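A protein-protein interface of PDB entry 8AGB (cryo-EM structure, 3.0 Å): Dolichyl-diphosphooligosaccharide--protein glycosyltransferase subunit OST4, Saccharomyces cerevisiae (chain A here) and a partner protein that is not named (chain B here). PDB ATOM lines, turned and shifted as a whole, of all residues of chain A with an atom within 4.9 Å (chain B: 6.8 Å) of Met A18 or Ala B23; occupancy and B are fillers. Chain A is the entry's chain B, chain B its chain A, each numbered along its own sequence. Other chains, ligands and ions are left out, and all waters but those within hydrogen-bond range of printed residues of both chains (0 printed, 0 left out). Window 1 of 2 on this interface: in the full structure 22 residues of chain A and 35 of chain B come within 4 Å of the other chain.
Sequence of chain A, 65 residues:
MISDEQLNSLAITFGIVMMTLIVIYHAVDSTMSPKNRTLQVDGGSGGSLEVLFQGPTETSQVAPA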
ATOM      1  N   THR A  13      -5.457   3.853  32.055  1.00  0.00           N
ATOM      2  CA  THR A  13      -4.661   5.074  32.001  1.00  0.00           C
ATOM      3  C   THR A  13      -3.773   5.095  30.765  1.00  0.00           C
ATOM      4  O   THR A  13      -3.653   6.129  30.097  1.00  0.00           O
ATOM      5  CB  THR A  13      -3.818   5.211  33.266  1.00  0.00           C
ATOM      6  OG1 THR A  13      -4.680   5.287  34.407  1.00  0.00           O
ATOM      7  CG2 THR A  13      -2.970   6.467  33.202  1.00  0.00           C
ATOM      8  N   PHE A  14      -3.136   3.964  30.453  1.00  0.00           N
ATOM      9  CA  PHE A  14      -2.341   3.873  29.234  1.00  0.00           C
ATOM     10  C   PHE A  14      -3.189   4.183  28.008  1.00  0.00           C
ATOM     11  O   PHE A  14      -2.781   4.960  27.136  1.00  0.00           O
ATOM     12  CB  PHE A  14      -1.719   2.482  29.120  1.00  0.00           C
ATOM     13  CG  PHE A  14      -0.322   2.395  29.660  1.00  0.00           C
ATOM     14  CD1 PHE A  14       0.619   3.354  29.338  1.00  0.00           C
ATOM     15  CD2 PHE A  14       0.051   1.349  30.482  1.00  0.00           C
ATOM     16  CE1 PHE A  14       1.904   3.274  29.829  1.00  0.00           C
ATOM     17  CE2 PHE A  14       1.334   1.264  30.975  1.00  0.00           C
ATOM     18  CZ  PHE A  14       2.261   2.228  30.648  1.00  0.00           C
ATOM     19  N   GLY A  15      -4.376   3.578  27.924  1.00  0.00           N
ATOM     20  CA  GLY A  15      -5.245   3.838  26.785  1.00  0.00           C
ATOM     21  C   GLY A  15      -5.646   5.296  26.665  1.00  0.00           C
ATOM     22  O   GLY A  15      -5.645   5.863  25.568  1.00  0.00           O
ATOM     23  N   ILE A  16      -5.991   5.925  27.791  1.00  0.00           N
ATOM     24  CA  ILE A  16      -6.440   7.314  27.750  1.00  0.00           C
ATOM     25  C   ILE A  16      -5.296   8.234  27.343  1.00  0.00           C
ATOM     26  O   ILE A  16      -5.475   9.150  26.531  1.00  0.00           O
ATOM     27  CB  ILE A  16      -7.042   7.723  29.105  1.00  0.00           C
ATOM     28  CG1 ILE A  16      -8.333   6.947  29.370  1.00  0.00           C
ATOM     29  CG2 ILE A  16      -7.291   9.220  29.150  1.00  0.00           C
ATOM     30  CD1 ILE A  16      -9.555   7.562  28.744  1.00  0.00           C
ATOM     31  N   VAL A  17      -4.100   7.995  27.885  1.00  0.00           N
ATOM     32  CA  VAL A  17      -2.946   8.812  27.519  1.00  0.00           C
ATOM     33  C   VAL A  17      -2.627   8.647  26.041  1.00  0.00           C
ATOM     34  O   VAL A  17      -2.322   9.623  25.344  1.00  0.00           O
ATOM     35  CB  VAL A  17      -1.736   8.461  28.404  1.00  0.00           C
ATOM     36  CG1 VAL A  17      -0.502   9.195  27.923  1.00  0.00           C
ATOM     37  CG2 VAL A  17      -2.022   8.816  29.849  1.00  0.00           C
ATOM     38  N   MET A  18      -2.700   7.414  25.536  1.00  0.00           N
ATOM     39  CA  MET A  18      -2.434   7.181  24.121  1.00  0.00           C
ATOM     40  C   MET A  18      -3.428   7.928  23.242  1.00  0.00           C
ATOM     41  O   MET A  18      -3.036   8.630  22.302  1.00  0.00           O
ATOM     42  CB  MET A  18      -2.475   5.681  23.830  1.00  0.00           C
ATOM     43  CG  MET A  18      -2.849   5.328  22.406  1.00  0.00           C
ATOM     44  SD  MET A  18      -2.838   3.551  22.115  1.00  0.00           S
ATOM     45  CE  MET A  18      -4.469   3.102  22.692  1.00  0.00           C
ATOM     46  N   MET A  19      -4.724   7.791  23.529  1.00  0.00           N
ATOM     47  CA  MET A  19      -5.721   8.444  22.687  1.00  0.00           C
ATOM     48  C   MET A  19      -5.701   9.962  22.817  1.00  0.00           C
ATOM     49  O   MET A  19      -5.966  10.658  21.829  1.00  0.00           O
ATOM     50  CB  MET A  19      -7.115   7.919  23.024  1.00  0.00           C
ATOM     51  CG  MET A  19      -7.380   6.513  22.528  1.00  0.00           C
ATOM     52  SD  MET A  19      -7.100   6.331  20.759  1.00  0.00           S
ATOM     53  CE  MET A  19      -7.705   4.669  20.501  1.00  0.00           C
ATOM     54  N   THR A  20      -5.201  10.491  23.931  1.00  0.00           N
ATOM     55  CA  THR A  20      -5.103  11.940  24.047  1.00  0.00           C
ATOM     56  C   THR A  20      -3.886  12.470  23.308  1.00  0.00           C
ATOM     57  O   THR A  20      -3.968  13.509  22.638  1.00  0.00           O
ATOM     58  CB  THR A  20      -5.065  12.342  25.522  1.00  0.00           C
ATOM     59  OG1 THR A  20      -6.399  12.367  26.043  1.00  0.00           O
ATOM     60  CG2 THR A  20      -4.437  13.712  25.698  1.00  0.00           C
ATOM     61  N   LEU A  21      -2.755  11.776  23.406  1.00  0.00           N
ATOM     62  CA  LEU A  21      -1.601  12.168  22.612  1.00  0.00           C
ATOM     63  C   LEU A  21      -1.916  12.091  21.123  1.00  0.00           C
ATOM     64  O   LEU A  21      -1.501  12.961  20.349  1.00  0.00           O
ATOM     65  CB  LEU A  21      -0.407  11.285  22.961  1.00  0.00           C
ATOM     66  CG  LEU A  21       0.159  11.494  24.362  1.00  0.00           C
ATOM     67  CD1 LEU A  21       1.113  10.374  24.715  1.00  0.00           C
ATOM     68  CD2 LEU A  21       0.851  12.841  24.452  1.00  0.00           C
ATOM     69  N   ILE A  22      -2.649  11.058  20.700  1.00  0.00           N
ATOM     70  CA  ILE A  22      -3.020  10.944  19.292  1.00  0.00           C
ATOM     71  C   ILE A  22      -3.903  12.110  18.864  1.00  0.00           C
ATOM     72  O   ILE A  22      -3.711  12.685  17.783  1.00  0.00           O
ATOM     73  CB  ILE A  22      -3.698   9.589  19.022  1.00  0.00           C
ATOM     74  CG1 ILE A  22      -2.677   8.457  19.122  1.00  0.00           C
ATOM     75  CG2 ILE A  22      -4.353   9.582  17.655  1.00  0.00           C
ATOM     76  CD1 ILE A  22      -3.289   7.082  19.073  1.00  0.00           C
ATOM     77  N   LEU B  18       7.257   9.463  19.124  1.00  0.00           N
ATOM     78  CA  LEU B  18       7.935   8.501  19.994  1.00  0.00           C
ATOM     79  C   LEU B  18       7.130   8.238  21.261  1.00  0.00           C
ATOM     80  O   LEU B  18       6.899   7.082  21.644  1.00  0.00           O
ATOM     81  CB  LEU B  18       9.340   8.998  20.340  1.00  0.00           C
ATOM     82  CG  LEU B  18      10.493   8.582  19.422  1.00  0.00           C
ATOM     83  CD1 LEU B  18      10.202   8.896  17.963  1.00  0.00           C
ATOM     84  CD2 LEU B  18      11.788   9.243  19.863  1.00  0.00           C
ATOM     85  N   VAL B  19       6.746   9.309  21.959  1.00  0.00           N
ATOM     86  CA  VAL B  19       5.958   9.159  23.182  1.00  0.00           C
ATOM     87  C   VAL B  19       4.700   8.345  22.899  1.00  0.00           C
ATOM     88  O   VAL B  19       4.307   7.467  23.683  1.00  0.00           O
ATOM     89  CB  VAL B  19       5.626  10.540  23.775  1.00  0.00           C
ATOM     90  CG1 VAL B  19       4.702  10.396  24.963  1.00  0.00           C
ATOM     91  CG2 VAL B  19       6.898  11.260  24.172  1.00  0.00           C
ATOM     92  N   ILE B  20       4.036   8.650  21.783  1.00  0.00           N
ATOM     93  CA  ILE B  20       2.826   7.929  21.399  1.00  0.00           C
ATOM     94  C   ILE B  20       3.121   6.442  21.279  1.00  0.00           C
ATOM     95  O   ILE B  20       2.350   5.602  21.752  1.00  0.00           O
ATOM     96  CB  ILE B  20       2.255   8.496  20.088  1.00  0.00           C
ATOM     97  CG1 ILE B  20       1.519   9.806  20.346  1.00  0.00           C
ATOM     98  CG2 ILE B  20       1.320   7.494  19.439  1.00  0.00           C
ATOM     99  CD1 ILE B  20       1.142  10.545  19.088  1.00  0.00           C
ATOM    100  N   PHE B  21       4.200   6.098  20.576  1.00  0.00           N
ATOM    101  CA  PHE B  21       4.524   4.690  20.372  1.00  0.00           C
ATOM    102  C   PHE B  21       5.019   4.010  21.638  1.00  0.00           C
ATOM    103  O   PHE B  21       5.119   2.782  21.658  1.00  0.00           O
ATOM    104  CB  PHE B  21       5.565   4.535  19.267  1.00  0.00           C
ATOM    105  CG  PHE B  21       4.967   4.328  17.914  1.00  0.00           C
ATOM    106  CD1 PHE B  21       4.274   3.168  17.627  1.00  0.00           C
ATOM    107  CD2 PHE B  21       5.084   5.294  16.935  1.00  0.00           C
ATOM    108  CE1 PHE B  21       3.715   2.972  16.388  1.00  0.00           C
ATOM    109  CE2 PHE B  21       4.526   5.101  15.694  1.00  0.00           C
ATOM    110  CZ  PHE B  21       3.840   3.939  15.420  1.00  0.00           C
ATOM    111  N   VAL B  22       5.325   4.769  22.683  1.00  0.00           N
ATOM    112  CA  VAL B  22       5.615   4.144  23.970  1.00  0.00           C
ATOM    113  C   VAL B  22       4.319   3.906  24.736  1.00  0.00           C
ATOM    114  O   VAL B  22       4.161   2.871  25.400  1.00  0.00           O
ATOM    115  CB  VAL B  22       6.598   4.992  24.795  1.00  0.00           C
ATOM    116  CG1 VAL B  22       6.886   4.319  26.120  1.00  0.00           C
ATOM    117  CG2 VAL B  22       7.888   5.193  24.026  1.00  0.00           C
ATOM    118  N   ALA B  23       3.335   4.778  24.525  1.00  0.00           N
ATOM    119  CA  ALA B  23       2.024   4.585  25.132  1.00  0.00           C
ATOM    120  C   ALA B  23       1.304   3.409  24.490  1.00  0.00           C
ATOM    121  O   ALA B  23       0.654   2.626  25.181  1.00  0.00           O
ATOM    122  CB  ALA B  23       1.195   5.861  25.011  1.00  0.00           C
ATOM    123  N   ILE B  24       1.310   3.344  23.158  1.00  0.00           N
ATOM    124  CA  ILE B  24       0.677   2.242  22.431  1.00  0.00           C
ATOM    125  C   ILE B  24       1.120   0.895  23.003  1.00  0.00           C
ATOM    126  O   ILE B  24       0.294   0.047  23.366  1.00  0.00           O
ATOM    127  CB  ILE B  24       0.989   2.339  20.928  1.00  0.00           C
ATOM    128  CG1 ILE B  24       0.204   3.486  20.295  1.00  0.00           C
ATOM    129  CG2 ILE B  24       0.658   1.034  20.232  1.00  0.00           C
ATOM    130  CD1 ILE B  24       0.472   3.662  18.824  1.00  0.00           C
ATOM    131  N   PHE B  25       2.434   0.651  22.989  1.00  0.00           N
ATOM    132  CA  PHE B  25       3.017  -0.528  23.625  1.00  0.00           C
ATOM    133  C   PHE B  25       2.507  -0.730  25.048  1.00  0.00           C
ATOM    134  O   PHE B  25       2.020  -1.815  25.398  1.00  0.00           O
ATOM    135  CB  PHE B  25       4.543  -0.427  23.616  1.00  0.00           C
ATOM    136  CG  PHE B  25       5.173  -0.910  22.344  1.00  0.00           C
ATOM    137  CD1 PHE B  25       5.099  -0.160  21.189  1.00  0.00           C
ATOM    138  CD2 PHE B  25       5.846  -2.117  22.308  1.00  0.00           C
ATOM    139  CE1 PHE B  25       5.680  -0.601  20.022  1.00  0.00           C
ATOM    140  CE2 PHE B  25       6.430  -2.565  21.144  1.00  0.00           C
ATOM    141  CZ  PHE B  25       6.346  -1.805  19.999  1.00  0.00           C
ATOM    142  N   GLY B  26       2.743   0.255  25.926  1.00  0.00           N
ATOM    143  CA  GLY B  26       2.284   0.116  27.301  1.00  0.00           C
ATOM    144  C   GLY B  26       0.828  -0.291  27.404  1.00  0.00           C
ATOM    145  O   GLY B  26       0.476  -1.182  28.182  1.00  0.00           O
ATOM    146  N   ALA B  27      -0.007   0.245  26.514  1.00  0.00           N
ATOM    147  CA  ALA B  27      -1.420  -0.113  26.464  1.00  0.00           C
ATOM    148  C   ALA B  27      -1.583  -1.585  26.143  1.00  0.00           C
ATOM    149  O   ALA B  27      -2.205  -2.327  26.904  1.00  0.00           O
ATOM    150  CB  ALA B  27      -2.146   0.753  25.434  1.00  0.00           C
ATOM    151  N   ALA B  28      -1.136  -1.992  24.956  1.00  0.00           N
ATOM    152  CA  ALA B  28      -1.349  -3.361  24.495  1.00  0.00           C
ATOM    153  C   ALA B  28      -0.878  -4.356  25.552  1.00  0.00           C
ATOM    154  O   ALA B  28      -1.654  -5.190  26.057  1.00  0.00           O
ATOM    155  CB  ALA B  28      -0.623  -3.585  23.169  1.00  0.00           C
ATOM    156  N   LEU B 144      -1.130   6.604  12.954  1.00  0.00           N
ATOM    157  CA  LEU B 144      -1.158   6.644  14.411  1.00  0.00           C
ATOM    158  C   LEU B 144      -2.523   6.235  14.943  1.00  0.00           C
ATOM    159  O   LEU B 144      -2.619   5.467  15.908  1.00  0.00           O
ATOM    160  CB  LEU B 144      -0.783   8.039  14.903  1.00  0.00           C
ATOM    161  CG  LEU B 144       0.710   8.366  14.879  1.00  0.00           C
ATOM    162  CD1 LEU B 144       0.946   9.787  15.330  1.00  0.00           C
ATOM    163  CD2 LEU B 144       1.484   7.393  15.746  1.00  0.00           C
ATOM    164  N   ALA B 147      -2.905   2.442  14.517  1.00  0.00           N
ATOM    165  CA  ALA B 147      -2.099   1.725  15.496  1.00  0.00           C
ATOM    166  C   ALA B 147      -2.746   1.777  16.870  1.00  0.00           C
ATOM    167  O   ALA B 147      -2.815   0.762  17.571  1.00  0.00           O
ATOM    168  CB  ALA B 147      -0.687   2.302  15.541  1.00  0.00           C
ATOM    169  N   GLY B 148      -3.246   2.950  17.264  1.00  0.00           N
ATOM    170  CA  GLY B 148      -3.930   3.055  18.541  1.00  0.00           C
ATOM    171  C   GLY B 148      -5.162   2.176  18.611  1.00  0.00           C
ATOM    172  O   GLY B 148      -5.425   1.538  19.632  1.00  0.00           O
ATOM    173  N   PHE B 149      -5.940   2.138  17.529  1.00  0.00           N
ATOM    174  CA  PHE B 149      -7.115   1.276  17.481  1.00  0.00           C
ATOM    175  C   PHE B 149      -6.727  -0.188  17.645  1.00  0.00           C
ATOM    176  O   PHE B 149      -7.206  -0.876  18.552  1.00  0.00           O
ATOM    177  CB  PHE B 149      -7.870   1.486  16.168  1.00  0.00           C
ATOM    178  CG  PHE B 149      -8.653   2.762  16.115  1.00  0.00           C
ATOM    179  CD1 PHE B 149      -9.101   3.364  17.274  1.00  0.00           C
ATOM    180  CD2 PHE B 149      -8.946   3.356  14.903  1.00  0.00           C
ATOM    181  CE1 PHE B 149      -9.822   4.536  17.223  1.00  0.00           C
ATOM    182  CE2 PHE B 149      -9.667   4.527  14.848  1.00  0.00           C
ATOM    183  CZ  PHE B 149     -10.104   5.118  16.009  1.00  0.00           C
ATOM    184  N   ALA B 151      -4.177  -1.518  18.783  1.00  0.00           N
ATOM    185  CA  ALA B 151      -3.416  -1.861  19.979  1.00  0.00           C
ATOM    186  C   ALA B 151      -4.276  -2.593  21.000  1.00  0.00           C
ATOM    187  O   ALA B 151      -3.798  -3.506  21.681  1.00  0.00           O
ATOM    188  CB  ALA B 151      -2.813  -0.601  20.594  1.00  0.00           C
ATOM    189  N   ILE B 152      -5.550  -2.213  21.121  1.00  0.00           N
ATOM    190  CA  ILE B 152      -6.399  -2.687  22.206  1.00  0.00           C
ATOM    191  C   ILE B 152      -7.739  -3.224  21.731  1.00  0.00           C
ATOM    192  O   ILE B 152      -8.568  -3.594  22.562  1.00  0.00           O
ATOM    193  CB  ILE B 152      -6.623  -1.584  23.262  1.00  0.00           C
ATOM    194  CG1 ILE B 152      -7.549  -0.501  22.708  1.00  0.00           C
ATOM    195  CG2 ILE B 152      -5.305  -0.988  23.716  1.00  0.00           C
ATOM    196  CD1 ILE B 152      -7.606   0.742  23.559  1.00  0.00           C
ATOM    197  N   PHE B 462     -14.693   4.054  23.654  1.00  0.00           N
ATOM    198  CA  PHE B 462     -14.143   2.858  23.026  1.00  0.00           C
ATOM    199  C   PHE B 462     -13.051   2.247  23.885  1.00  0.00           C
ATOM    200  O   PHE B 462     -12.980   1.023  24.033  1.00  0.00           O
ATOM    201  CB  PHE B 462     -13.615   3.198  21.631  1.00  0.00           C
ATOM    202  CG  PHE B 462     -12.658   2.182  21.072  1.00  0.00           C
ATOM    203  CD1 PHE B 462     -13.126   1.052  20.432  1.00  0.00           C
ATOM    204  CD2 PHE B 462     -11.291   2.377  21.155  1.00  0.00           C
ATOM    205  CE1 PHE B 462     -12.251   0.123  19.909  1.00  0.00           C
ATOM    206  CE2 PHE B 462     -10.414   1.449  20.633  1.00  0.00           C
ATOM    207  CZ  PHE B 462     -10.894   0.323  20.009  1.00  0.00           C
ATOM    208  N   VAL B 463     -12.179   3.084  24.448  1.00  0.00           N
ATOM    209  CA  VAL B 463     -11.131   2.575  25.333  1.00  0.00           C
ATOM    210  C   VAL B 463     -11.747   1.828  26.512  1.00  0.00           C
ATOM    211  O   VAL B 463     -11.330   0.715  26.859  1.00  0.00           O
ATOM    212  CB  VAL B 463     -10.222   3.722  25.807  1.00  0.00           C
ATOM    213  CG1 VAL B 463      -9.398   3.284  27.003  1.00  0.00           C
ATOM    214  CG2 VAL B 463      -9.322   4.179  24.678  1.00  0.00           C
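Of chain B, only Ala B23 (3.9 Å), Ile B24 (3.5 Å) and Gly B148 (3.6 Å) come within 4 Å of Met A18. Of the printed residues of chain B, Ile A22 touches Leu B144. Val B22 touches none of the printed residues of chain A. Of chain A, only Met A18 comes within 4 Å of Ala B23. Of the printed residues of chain A, Gly B26 touches Phe A14 (3.4 Å). Ala B151 touches none of the printed residues of chain A. The nearest residue of chain A that does not touch Ala B23 is Phe A14 (4.2 Å). The nearest printed residue of chain A that does not touch Val B463 is Gly A15 (4.1 Å).
Among the printed residues, pairs that only touch across the chains: Phe A14 with Gly B26 (3.4 Å), Phe A14 with Ala B27 (3.7 Å), Met A18 with Ala B23 (3.9 Å), Met A18 with Ile B24 (3.5 Å), Met A18 with Gly B148 (3.6 Å), Met A19 with Gly B148 (3.97 Å), Met A19 with Phe B149 (3.8 Å), Met A19 with Val B463 (3.7 Å), Leu A21 with Val B19 (3.6 Å), Leu A21 with Ile B20 (3.6 Å) and Ile A22 with Leu B144 (3.6 Å).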
